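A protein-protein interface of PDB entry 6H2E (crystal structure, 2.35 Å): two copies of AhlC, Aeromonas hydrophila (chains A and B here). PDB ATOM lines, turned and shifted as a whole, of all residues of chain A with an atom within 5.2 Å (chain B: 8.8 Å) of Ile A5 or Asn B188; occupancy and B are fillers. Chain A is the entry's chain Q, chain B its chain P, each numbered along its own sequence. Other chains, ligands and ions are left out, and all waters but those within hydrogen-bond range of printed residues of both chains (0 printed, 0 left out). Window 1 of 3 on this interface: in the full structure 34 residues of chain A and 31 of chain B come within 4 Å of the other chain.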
ATOM      1  N   ASN A   3      27.140  12.640  14.271  1.00  0.00           N
ATOM      2  CA  ASN A   3      26.899  11.389  15.063  1.00  0.00           C
ATOM      3  C   ASN A   3      25.643  10.679  14.518  1.00  0.00           C
ATOM      4  O   ASN A   3      24.653  11.326  14.214  1.00  0.00           O
ATOM      5  CB  ASN A   3      26.827  11.693  16.562  1.00  0.00           C
ATOM      6  CG  ASN A   3      28.006  11.234  17.420  1.00  0.00           C
ATOM      7  OD1 ASN A   3      29.046  10.754  16.942  1.00  0.00           O
ATOM      8  ND2 ASN A   3      27.857  11.404  18.730  1.00  0.00           N
ATOM      9  N   GLY A   4      25.725   9.354  14.307  1.00  0.00           N
ATOM     10  CA  GLY A   4      24.583   8.519  13.820  1.00  0.00           C
ATOM     11  C   GLY A   4      23.599   8.166  14.943  1.00  0.00           C
ATOM     12  O   GLY A   4      23.767   8.602  16.109  1.00  0.00           O
ATOM     13  N   ILE A   5      22.592   7.339  14.634  1.00  0.00           N
ATOM     14  CA  ILE A   5      21.437   7.141  15.543  1.00  0.00           C
ATOM     15  C   ILE A   5      21.857   6.460  16.849  1.00  0.00           C
ATOM     16  O   ILE A   5      21.507   6.923  17.937  1.00  0.00           O
ATOM     17  CB  ILE A   5      20.266   6.393  14.871  1.00  0.00           C
ATOM     18  CG1 ILE A   5      19.678   7.272  13.771  1.00  0.00           C
ATOM     19  CG2 ILE A   5      19.182   5.964  15.902  1.00  0.00           C
ATOM     20  CD1 ILE A   5      18.949   8.497  14.269  1.00  0.00           C
ATOM     21  N   LEU A   6      22.547   5.341  16.731  1.00  0.00           N
ATOM     22  CA  LEU A   6      23.109   4.679  17.894  1.00  0.00           C
ATOM     23  C   LEU A   6      23.879   5.660  18.768  1.00  0.00           C
ATOM     24  O   LEU A   6      23.667   5.730  19.975  1.00  0.00           O
ATOM     25  CB  LEU A   6      24.023   3.552  17.432  1.00  0.00           C
ATOM     26  CG  LEU A   6      23.317   2.268  17.041  1.00  0.00           C
ATOM     27  CD1 LEU A   6      24.344   1.232  16.599  1.00  0.00           C
ATOM     28  CD2 LEU A   6      22.513   1.728  18.206  1.00  0.00           C
ATOM     29  N   SER A   7      24.759   6.432  18.141  1.00  0.00           N
ATOM     30  CA  SER A   7      25.639   7.281  18.857  1.00  0.00           C
ATOM     31  C   SER A   7      24.890   8.470  19.415  1.00  0.00           C
ATOM     32  O   SER A   7      25.225   8.918  20.460  1.00  0.00           O
ATOM     33  CB  SER A   7      26.785   7.717  18.015  1.00  0.00           C
ATOM     34  OG  SER A   7      27.551   6.598  17.676  1.00  0.00           O
ATOM     35  N   GLN A   8      23.861   8.977  18.737  1.00  0.00           N
ATOM     36  CA  GLN A   8      23.132  10.084  19.379  1.00  0.00           C
ATOM     37  C   GLN A   8      22.346   9.561  20.593  1.00  0.00           C
ATOM     38  O   GLN A   8      22.243  10.233  21.619  1.00  0.00           O
ATOM     39  CB  GLN A   8      22.179  10.748  18.409  1.00  0.00           C
ATOM     40  CG  GLN A   8      22.880  11.544  17.340  1.00  0.00           C
ATOM     41  CD  GLN A   8      21.802  12.049  16.424  1.00  0.00           C
ATOM     42  OE1 GLN A   8      20.739  12.443  16.900  1.00  0.00           O
ATOM     43  NE2 GLN A   8      22.063  11.997  15.126  1.00  0.00           N
ATOM     44  N   SER A   9      21.720   8.392  20.427  1.00  0.00           N
ATOM     45  CA  SER A   9      20.916   7.804  21.493  1.00  0.00           C
ATOM     46  C   SER A   9      21.811   7.632  22.718  1.00  0.00           C
ATOM     47  O   SER A   9      21.454   8.047  23.778  1.00  0.00           O
ATOM     48  CB  SER A   9      20.321   6.476  21.057  1.00  0.00           C
ATOM     49  OG  SER A   9      19.477   6.687  19.942  1.00  0.00           O
ATOM     50  N   ILE A  10      22.952   6.963  22.539  1.00  0.00           N
ATOM     51  CA  ILE A  10      23.920   6.764  23.660  1.00  0.00           C
ATOM     52  C   ILE A  10      24.184   8.112  24.309  1.00  0.00           C
ATOM     53  O   ILE A  10      23.902   8.306  25.514  1.00  0.00           O
ATOM     54  CB  ILE A  10      25.200   6.052  23.201  1.00  0.00           C
ATOM     55  CG1 ILE A  10      24.882   4.596  22.892  1.00  0.00           C
ATOM     56  CG2 ILE A  10      26.334   6.176  24.223  1.00  0.00           C
ATOM     57  CD1 ILE A  10      25.891   3.911  21.984  1.00  0.00           C
ATOM     58  N   ASN A  12      22.543  10.889  24.203  1.00  0.00           N
ATOM     59  CA  ASN A  12      21.349  11.527  24.847  1.00  0.00           C
ATOM     60  C   ASN A  12      21.047  10.771  26.150  1.00  0.00           C
ATOM     61  O   ASN A  12      20.726  11.380  27.149  1.00  0.00           O
ATOM     62  CB  ASN A  12      20.133  11.644  23.927  1.00  0.00           C
ATOM     63  CG  ASN A  12      20.327  12.581  22.740  1.00  0.00           C
ATOM     64  OD1 ASN A  12      20.968  13.613  22.841  1.00  0.00           O
ATOM     65  ND2 ASN A  12      19.703  12.283  21.613  1.00  0.00           N
ATOM     66  N   GLN A 210      14.633   7.710  24.035  1.00  0.00           N
ATOM     67  CA  GLN A 210      15.973   7.527  23.501  1.00  0.00           C
ATOM     68  C   GLN A 210      16.318   6.047  23.440  1.00  0.00           C
ATOM     69  O   GLN A 210      16.840   5.579  22.435  1.00  0.00           O
ATOM     70  CB  GLN A 210      17.008   8.280  24.339  1.00  0.00           C
ATOM     71  CG  GLN A 210      16.858   9.786  24.241  1.00  0.00           C
ATOM     72  CD  GLN A 210      17.150  10.407  22.890  1.00  0.00           C
ATOM     73  OE1 GLN A 210      17.880   9.874  22.068  1.00  0.00           O
ATOM     74  NE2 GLN A 210      16.646  11.621  22.702  1.00  0.00           N
ATOM     75  N   SER A 213      14.542   4.304  20.676  1.00  0.00           N
ATOM     76  CA  SER A 213      15.246   4.547  19.366  1.00  0.00           C
ATOM     77  C   SER A 213      16.422   3.577  19.254  1.00  0.00           C
ATOM     78  O   SER A 213      16.651   2.993  18.225  1.00  0.00           O
ATOM     79  CB  SER A 213      15.713   5.996  19.174  1.00  0.00           C
ATOM     80  OG  SER A 213      14.623   6.903  19.239  1.00  0.00           O
ATOM     81  N   ARG A 217      16.942   0.493  16.564  1.00  0.00           N
ATOM     82  CA  ARG A 217      18.110   0.400  15.674  1.00  0.00           C
ATOM     83  C   ARG A 217      18.828  -0.942  15.844  1.00  0.00           C
ATOM     84  O   ARG A 217      19.303  -1.558  14.911  1.00  0.00           O
ATOM     85  CB  ARG A 217      19.122   1.522  15.942  1.00  0.00           C
ATOM     86  CG  ARG A 217      20.275   1.551  14.943  1.00  0.00           C
ATOM     87  CD  ARG A 217      19.913   1.307  13.478  1.00  0.00           C
ATOM     88  NE  ARG A 217      18.990   2.263  12.878  1.00  0.00           N
ATOM     89  CZ  ARG A 217      19.295   3.378  12.199  1.00  0.00           C
ATOM     90  NH1 ARG A 217      20.549   3.789  12.068  1.00  0.00           N
ATOM     91  NH2 ARG A 217      18.308   4.105  11.685  1.00  0.00           N
ATOM     92  N   ILE B 131      12.852  21.522  11.767  1.00  0.00           N
ATOM     93  CA  ILE B 131      12.454  20.108  11.573  1.00  0.00           C
ATOM     94  C   ILE B 131      11.430  19.971  10.444  1.00  0.00           C
ATOM     95  O   ILE B 131      11.521  19.090   9.598  1.00  0.00           O
ATOM     96  CB  ILE B 131      11.875  19.470  12.841  1.00  0.00           C
ATOM     97  CG1 ILE B 131      12.963  19.211  13.876  1.00  0.00           C
ATOM     98  CG2 ILE B 131      11.110  18.197  12.479  1.00  0.00           C
ATOM     99  CD1 ILE B 131      12.452  18.447  15.060  1.00  0.00           C
ATOM    100  N   LEU B 134      12.968  19.517   7.044  1.00  0.00           N
ATOM    101  CA  LEU B 134      13.829  18.355   6.826  1.00  0.00           C
ATOM    102  C   LEU B 134      12.981  17.069   6.827  1.00  0.00           C
ATOM    103  O   LEU B 134      13.218  16.198   6.006  1.00  0.00           O
ATOM    104  CB  LEU B 134      14.912  18.254   7.910  1.00  0.00           C
ATOM    105  CG  LEU B 134      15.999  19.333   7.973  1.00  0.00           C
ATOM    106  CD1 LEU B 134      16.764  19.183   9.292  1.00  0.00           C
ATOM    107  CD2 LEU B 134      16.970  19.253   6.805  1.00  0.00           C
ATOM    108  N   GLN B 135      12.086  16.929   7.816  1.00  0.00           N
ATOM    109  CA  GLN B 135      11.071  15.859   7.932  1.00  0.00           C
ATOM    110  C   GLN B 135      10.369  15.667   6.577  1.00  0.00           C
ATOM    111  O   GLN B 135      10.310  14.554   6.055  1.00  0.00           O
ATOM    112  CB  GLN B 135      10.091  16.194   9.064  1.00  0.00           C
ATOM    113  CG  GLN B 135       9.189  15.039   9.477  1.00  0.00           C
ATOM    114  CD  GLN B 135       9.928  13.851  10.049  1.00  0.00           C
ATOM    115  OE1 GLN B 135      10.432  13.886  11.171  1.00  0.00           O
ATOM    116  NE2 GLN B 135       9.949  12.762   9.295  1.00  0.00           N
ATOM    117  N   LEU B 138      12.648  13.820   4.475  1.00  0.00           N
ATOM    118  CA  LEU B 138      12.919  12.535   5.051  1.00  0.00           C
ATOM    119  C   LEU B 138      11.799  11.572   4.659  1.00  0.00           C
ATOM    120  O   LEU B 138      12.073  10.495   4.143  1.00  0.00           O
ATOM    121  CB  LEU B 138      13.048  12.680   6.576  1.00  0.00           C
ATOM    122  CG  LEU B 138      13.195  11.373   7.365  1.00  0.00           C
ATOM    123  CD1 LEU B 138      14.280  10.499   6.777  1.00  0.00           C
ATOM    124  CD2 LEU B 138      13.506  11.650   8.832  1.00  0.00           C
ATOM    125  N   ARG B 142      12.097   8.124   2.601  1.00  0.00           N
ATOM    126  CA  ARG B 142      11.661   6.898   3.263  1.00  0.00           C
ATOM    127  C   ARG B 142      10.633   6.154   2.404  1.00  0.00           C
ATOM    128  O   ARG B 142      10.698   4.924   2.257  1.00  0.00           O
ATOM    129  CB  ARG B 142      11.127   7.257   4.650  1.00  0.00           C
ATOM    130  CG  ARG B 142      11.982   6.794   5.818  1.00  0.00           C
ATOM    131  CD  ARG B 142      11.568   7.483   7.107  1.00  0.00           C
ATOM    132  NE  ARG B 142      12.440   7.183   8.229  1.00  0.00           N
ATOM    133  CZ  ARG B 142      12.394   7.817   9.408  1.00  0.00           C
ATOM    134  NH1 ARG B 142      11.388   8.640   9.709  1.00  0.00           N
ATOM    135  NH2 ARG B 142      13.379   7.637  10.273  1.00  0.00           N
ATOM    136  N   VAL B 180      18.678   9.008   3.451  1.00  0.00           N
ATOM    137  CA  VAL B 180      17.813   8.790   4.622  1.00  0.00           C
ATOM    138  C   VAL B 180      18.656   8.928   5.889  1.00  0.00           C
ATOM    139  O   VAL B 180      18.291   9.670   6.759  1.00  0.00           O
ATOM    140  CB  VAL B 180      17.096   7.432   4.573  1.00  0.00           C
ATOM    141  CG1 VAL B 180      16.490   7.030   5.929  1.00  0.00           C
ATOM    142  CG2 VAL B 180      16.033   7.445   3.508  1.00  0.00           C
ATOM    143  N   SER B 181      19.782   8.206   5.951  1.00  0.00           N
ATOM    144  CA  SER B 181      20.717   8.212   7.113  1.00  0.00           C
ATOM    145  C   SER B 181      21.005   9.622   7.586  1.00  0.00           C
ATOM    146  O   SER B 181      20.987   9.884   8.762  1.00  0.00           O
ATOM    147  CB  SER B 181      22.029   7.546   6.780  1.00  0.00           C
ATOM    148  OG  SER B 181      23.045   7.913   7.713  1.00  0.00           O
ATOM    149  N   SER B 182      21.326  10.482   6.625  1.00  0.00           N
ATOM    150  CA  SER B 182      21.790  11.840   6.863  1.00  0.00           C
ATOM    151  C   SER B 182      20.620  12.716   7.312  1.00  0.00           C
ATOM    152  O   SER B 182      20.782  13.540   8.234  1.00  0.00           O
ATOM    153  CB  SER B 182      22.467  12.414   5.629  1.00  0.00           C
ATOM    154  OG  SER B 182      22.633  13.823   5.734  1.00  0.00           O
ATOM    155  N   LEU B 183      19.457  12.547   6.662  1.00  0.00           N
ATOM    156  CA  LEU B 183      18.264  13.315   7.036  1.00  0.00           C
ATOM    157  C   LEU B 183      17.728  12.890   8.407  1.00  0.00           C
ATOM    158  O   LEU B 183      17.332  13.740   9.192  1.00  0.00           O
ATOM    159  CB  LEU B 183      17.180  13.200   5.974  1.00  0.00           C
ATOM    160  CG  LEU B 183      17.488  13.923   4.667  1.00  0.00           C
ATOM    161  CD1 LEU B 183      16.432  13.618   3.621  1.00  0.00           C
ATOM    162  CD2 LEU B 183      17.605  15.420   4.895  1.00  0.00           C
ATOM    163  N   GLU B 184      17.709  11.593   8.680  1.00  0.00           N
ATOM    164  CA  GLU B 184      17.185  11.051   9.952  1.00  0.00           C
ATOM    165  C   GLU B 184      18.144  11.462  11.073  1.00  0.00           C
ATOM    166  O   GLU B 184      17.730  11.893  12.091  1.00  0.00           O
ATOM    167  CB  GLU B 184      16.980   9.548   9.747  1.00  0.00           C
ATOM    168  CG  GLU B 184      17.307   8.618  10.901  1.00  0.00           C
ATOM    169  CD  GLU B 184      17.216   7.148  10.480  1.00  0.00           C
ATOM    170  OE1 GLU B 184      18.302   6.471  10.362  1.00  0.00           O
ATOM    171  OE2 GLU B 184      16.064   6.681  10.234  1.00  0.00           O
ATOM    172  N   GLY B 185      19.448  11.344  10.819  1.00  0.00           N
ATOM    173  CA  GLY B 185      20.485  11.854  11.695  1.00  0.00           C
ATOM    174  C   GLY B 185      20.267  13.301  12.114  1.00  0.00           C
ATOM    175  O   GLY B 185      20.426  13.619  13.271  1.00  0.00           O
ATOM    176  N   GLN B 186      19.938  14.183  11.169  1.00  0.00           N
ATOM    177  CA  GLN B 186      19.838  15.615  11.451  1.00  0.00           C
ATOM    178  C   GLN B 186      18.534  15.892  12.204  1.00  0.00           C
ATOM    179  O   GLN B 186      18.512  16.706  13.102  1.00  0.00           O
ATOM    180  CB  GLN B 186      19.784  16.483  10.191  1.00  0.00           C
ATOM    181  CG  GLN B 186      21.105  16.719   9.472  1.00  0.00           C
ATOM    182  CD  GLN B 186      20.831  17.324   8.106  1.00  0.00           C
ATOM    183  OE1 GLN B 186      21.185  16.760   7.076  1.00  0.00           O
ATOM    184  NE2 GLN B 186      20.134  18.450   8.069  1.00  0.00           N
ATOM    185  N   VAL B 187      17.446  15.225  11.789  1.00  0.00           N
ATOM    186  CA  VAL B 187      16.176  15.376  12.430  1.00  0.00           C
ATOM    187  C   VAL B 187      16.283  14.912  13.888  1.00  0.00           C
ATOM    188  O   VAL B 187      15.760  15.565  14.759  1.00  0.00           O
ATOM    189  CB  VAL B 187      15.070  14.635  11.657  1.00  0.00           C
ATOM    190  CG1 VAL B 187      13.817  14.349  12.506  1.00  0.00           C
ATOM    191  CG2 VAL B 187      14.722  15.431  10.415  1.00  0.00           C
ATOM    192  N   ASN B 188      16.945  13.782  14.140  1.00  0.00           N
ATOM    193  CA  ASN B 188      17.088  13.223  15.526  1.00  0.00           C
ATOM    194  C   ASN B 188      17.923  14.168  16.412  1.00  0.00           C
ATOM    195  O   ASN B 188      17.578  14.442  17.552  1.00  0.00           O
ATOM    196  CB  ASN B 188      17.660  11.804  15.488  1.00  0.00           C
ATOM    197  CG  ASN B 188      17.337  10.978  16.712  1.00  0.00           C
ATOM    198  OD1 ASN B 188      16.221  10.506  16.868  1.00  0.00           O
ATOM    199  ND2 ASN B 188      18.332  10.719  17.541  1.00  0.00           N
ATOM    200  N   GLN B 189      18.999  14.742  15.879  1.00  0.00           N
ATOM    201  CA  GLN B 189      19.816  15.695  16.663  1.00  0.00           C
ATOM    202  C   GLN B 189      18.964  16.874  17.168  1.00  0.00           C
ATOM    203  O   GLN B 189      19.078  17.306  18.341  1.00  0.00           O
ATOM    204  CB  GLN B 189      21.022  16.186  15.851  1.00  0.00           C
ATOM    205  CG  GLN B 189      21.997  17.051  16.657  1.00  0.00           C
ATOM    206  CD  GLN B 189      22.874  16.249  17.588  1.00  0.00           C
ATOM    207  OE1 GLN B 189      23.774  15.512  17.169  1.00  0.00           O
ATOM    208  NE2 GLN B 189      22.653  16.428  18.882  1.00  0.00           N
ATOM    209  N   ILE B 190      18.128  17.422  16.287  1.00  0.00           N
ATOM    210  CA  ILE B 190      17.317  18.566  16.604  1.00  0.00           C
ATOM    211  C   ILE B 190      16.214  18.183  17.607  1.00  0.00           C
ATOM    212  O   ILE B 190      15.902  18.965  18.487  1.00  0.00           O
ATOM    213  CB  ILE B 190      16.743  19.184  15.313  1.00  0.00           C
ATOM    214  CG1 ILE B 190      17.844  19.826  14.465  1.00  0.00           C
ATOM    215  CG2 ILE B 190      15.625  20.168  15.620  1.00  0.00           C
ATOM    216  CD1 ILE B 190      17.331  20.499  13.204  1.00  0.00           C
ATOM    217  N   GLU B 191      15.597  17.013  17.430  1.00  0.00           N
ATOM    218  CA  GLU B 191      14.579  16.481  18.361  1.00  0.00           C
ATOM    219  C   GLU B 191      15.209  16.329  19.756  1.00  0.00           C
ATOM    220  O   GLU B 191      14.563  16.618  20.744  1.00  0.00           O
ATOM    221  CB  GLU B 191      13.946  15.180  17.849  1.00  0.00           C
ATOM    222  CG  GLU B 191      12.906  15.408  16.739  1.00  0.00           C
ATOM    223  CD  GLU B 191      12.114  14.212  16.188  1.00  0.00           C
ATOM    224  OE1 GLU B 191      12.451  13.050  16.533  1.00  0.00           O
ATOM    225  OE2 GLU B 191      11.131  14.441  15.414  1.00  0.00           O
ATOM    226  N   GLY B 192      16.489  15.975  19.816  1.00  0.00           N
ATOM    227  CA  GLY B 192      17.230  15.805  21.059  1.00  0.00           C
ATOM    228  C   GLY B 192      17.363  17.112  21.813  1.00  0.00           C
ATOM    229  O   GLY B 192      17.155  17.140  23.019  1.00  0.00           O
ATOM    230  N   GLN B 193      17.703  18.176  21.074  1.00  0.00           N
ATOM    231  CA  GLN B 193      17.850  19.494  21.563  1.00  0.00           C
ATOM    232  C   GLN B 193      16.509  19.986  22.110  1.00  0.00           C
ATOM    233  O   GLN B 193      16.433  20.600  23.162  1.00  0.00           O
ATOM    234  CB  GLN B 193      18.333  20.464  20.469  1.00  0.00           C
ATOM    235  CG  GLN B 193      19.846  20.540  20.291  1.00  0.00           C
ATOM    236  CD  GLN B 193      20.270  20.773  18.853  1.00  0.00           C
ATOM    237  OE1 GLN B 193      19.712  21.588  18.122  1.00  0.00           O
ATOM    238  NE2 GLN B 193      21.280  20.035  18.423  1.00  0.00           N
ATOM    239  N   ILE B 194      15.442  19.737  21.378  1.00  0.00           N
ATOM    240  CA  ILE B 194      14.166  20.253  21.819  1.00  0.00           C
ATOM    241  C   ILE B 194      13.786  19.570  23.129  1.00  0.00           C
ATOM    242  O   ILE B 194      13.455  20.240  24.080  1.00  0.00           O
ATOM    243  CB  ILE B 194      13.101  20.078  20.737  1.00  0.00           C
ATOM    244  CG1 ILE B 194      13.354  21.045  19.575  1.00  0.00           C
ATOM    245  CG2 ILE B 194      11.715  20.244  21.344  1.00  0.00           C
ATOM    246  CD1 ILE B 194      12.506  20.732  18.343  1.00  0.00           C
ATOM    247  N   GLN B 195      14.013  18.258  23.176  1.00  0.00           N
ATOM    248  CA  GLN B 195      13.712  17.422  24.312  1.00  0.00           C
ATOM    249  C   GLN B 195      14.480  17.913  25.554  1.00  0.00           C
ATOM    250  O   GLN B 195      13.886  18.154  26.516  1.00  0.00           O
ATOM    251  CB  GLN B 195      14.038  15.971  23.977  1.00  0.00           C
ATOM    252  CG  GLN B 195      13.255  14.953  24.791  1.00  0.00           C
ATOM    253  CD  GLN B 195      13.563  13.547  24.330  1.00  0.00           C
ATOM    254  OE1 GLN B 195      12.675  12.764  23.975  1.00  0.00           O
ATOM    255  NE2 GLN B 195      14.842  13.225  24.326  1.00  0.00           N
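Along chain A the printed residues that touch a printed residue of chain B span positions 5 to 217. Among the printed residues, Asp or Glu carboxylates within 4 Å of a Lys or Arg side-chain nitrogen of the other chain: Arg A217 with Glu B184 (2.7 Å).
No position is printed for both chains. Of the 7 pairs that touch across the chains among the printed residues, none has its exchanged pair printed and touching as well.
NE2 of Gln A8 lies within hydrogen-bond range of O of Asn A3 (2.8 Å). The side-chain amide nitrogen (ND2) of Asn A12 is in hydrogen-bond range of the side-chain amide oxygen (OE1) of Gln A210. The backbone carbonyl oxygen (O) of Ile A5 is in hydrogen-bond range of the side-chain hydroxyl (OG) of Ser A9 (2.9 Å). The side-chain amide nitrogen of Asn A12 lies close to the backbone carbonyl oxygen of Gln A8, at 3.3 Å. The side-chain carboxylate (OE2) of Glu B184 lies within salt-bridge range of the guanidinium group (NH2) of Arg B142, 2.9 Å away.
Ile A5 touches Glu B184 (CD1 to CG, 3.7 Å). Asn B188 touches Ile A5 (CB to CD1, 3.8 Å).
Ile A5 touches two residues of chain B. Of the printed residues of chain A, Asn B188 touches Ile A5 and Gln A8. No residue of chain B comes within 4 Å of Gly A4. Printed residues of chain A within 4 Å of Glu B184: Ile A5 (3.7 Å) and Arg A217 (2.7 Å). Of the printed residues of chain B, Gln A8 touches Gly B185 (3.0 Å), Asn B188 (3.0 Å) and Gln B189 (3.1 Å). Printed residues of chain B within 4 Å of Gln A210: Gln B195. Of the printed residues of chain A, Gln B189 touches Gln A8. Of the printed residues of chain B, Arg A217 touches Glu B184 (2.7 Å). Leu B138 touches none of the printed residues of chain A. The nearest printed residue of chain A that does not touch Gln B195 is Asn A12 (5.5 Å).
The backbone NH (N) of Gln B189 lies within hydrogen-bond range of the side-chain amide oxygen (OE1) of Gln A8, at 3.1 Å. The side-chain amide nitrogen of Gln B195 sits close to the side-chain amide nitrogen of Gln A210 (2.9 Å). O of Gly B185 sits at hydrogen-bond distance from NE2 of Gln A8, at 3.0 Å. OE1 of Gln A8 is in hydrogen-bond range of ND2 of Asn B188 (3.0 Å). The guanidinium group of Arg A217 is in salt-bridge range of the side-chain carboxylate of Glu B184 (2.7 Å).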
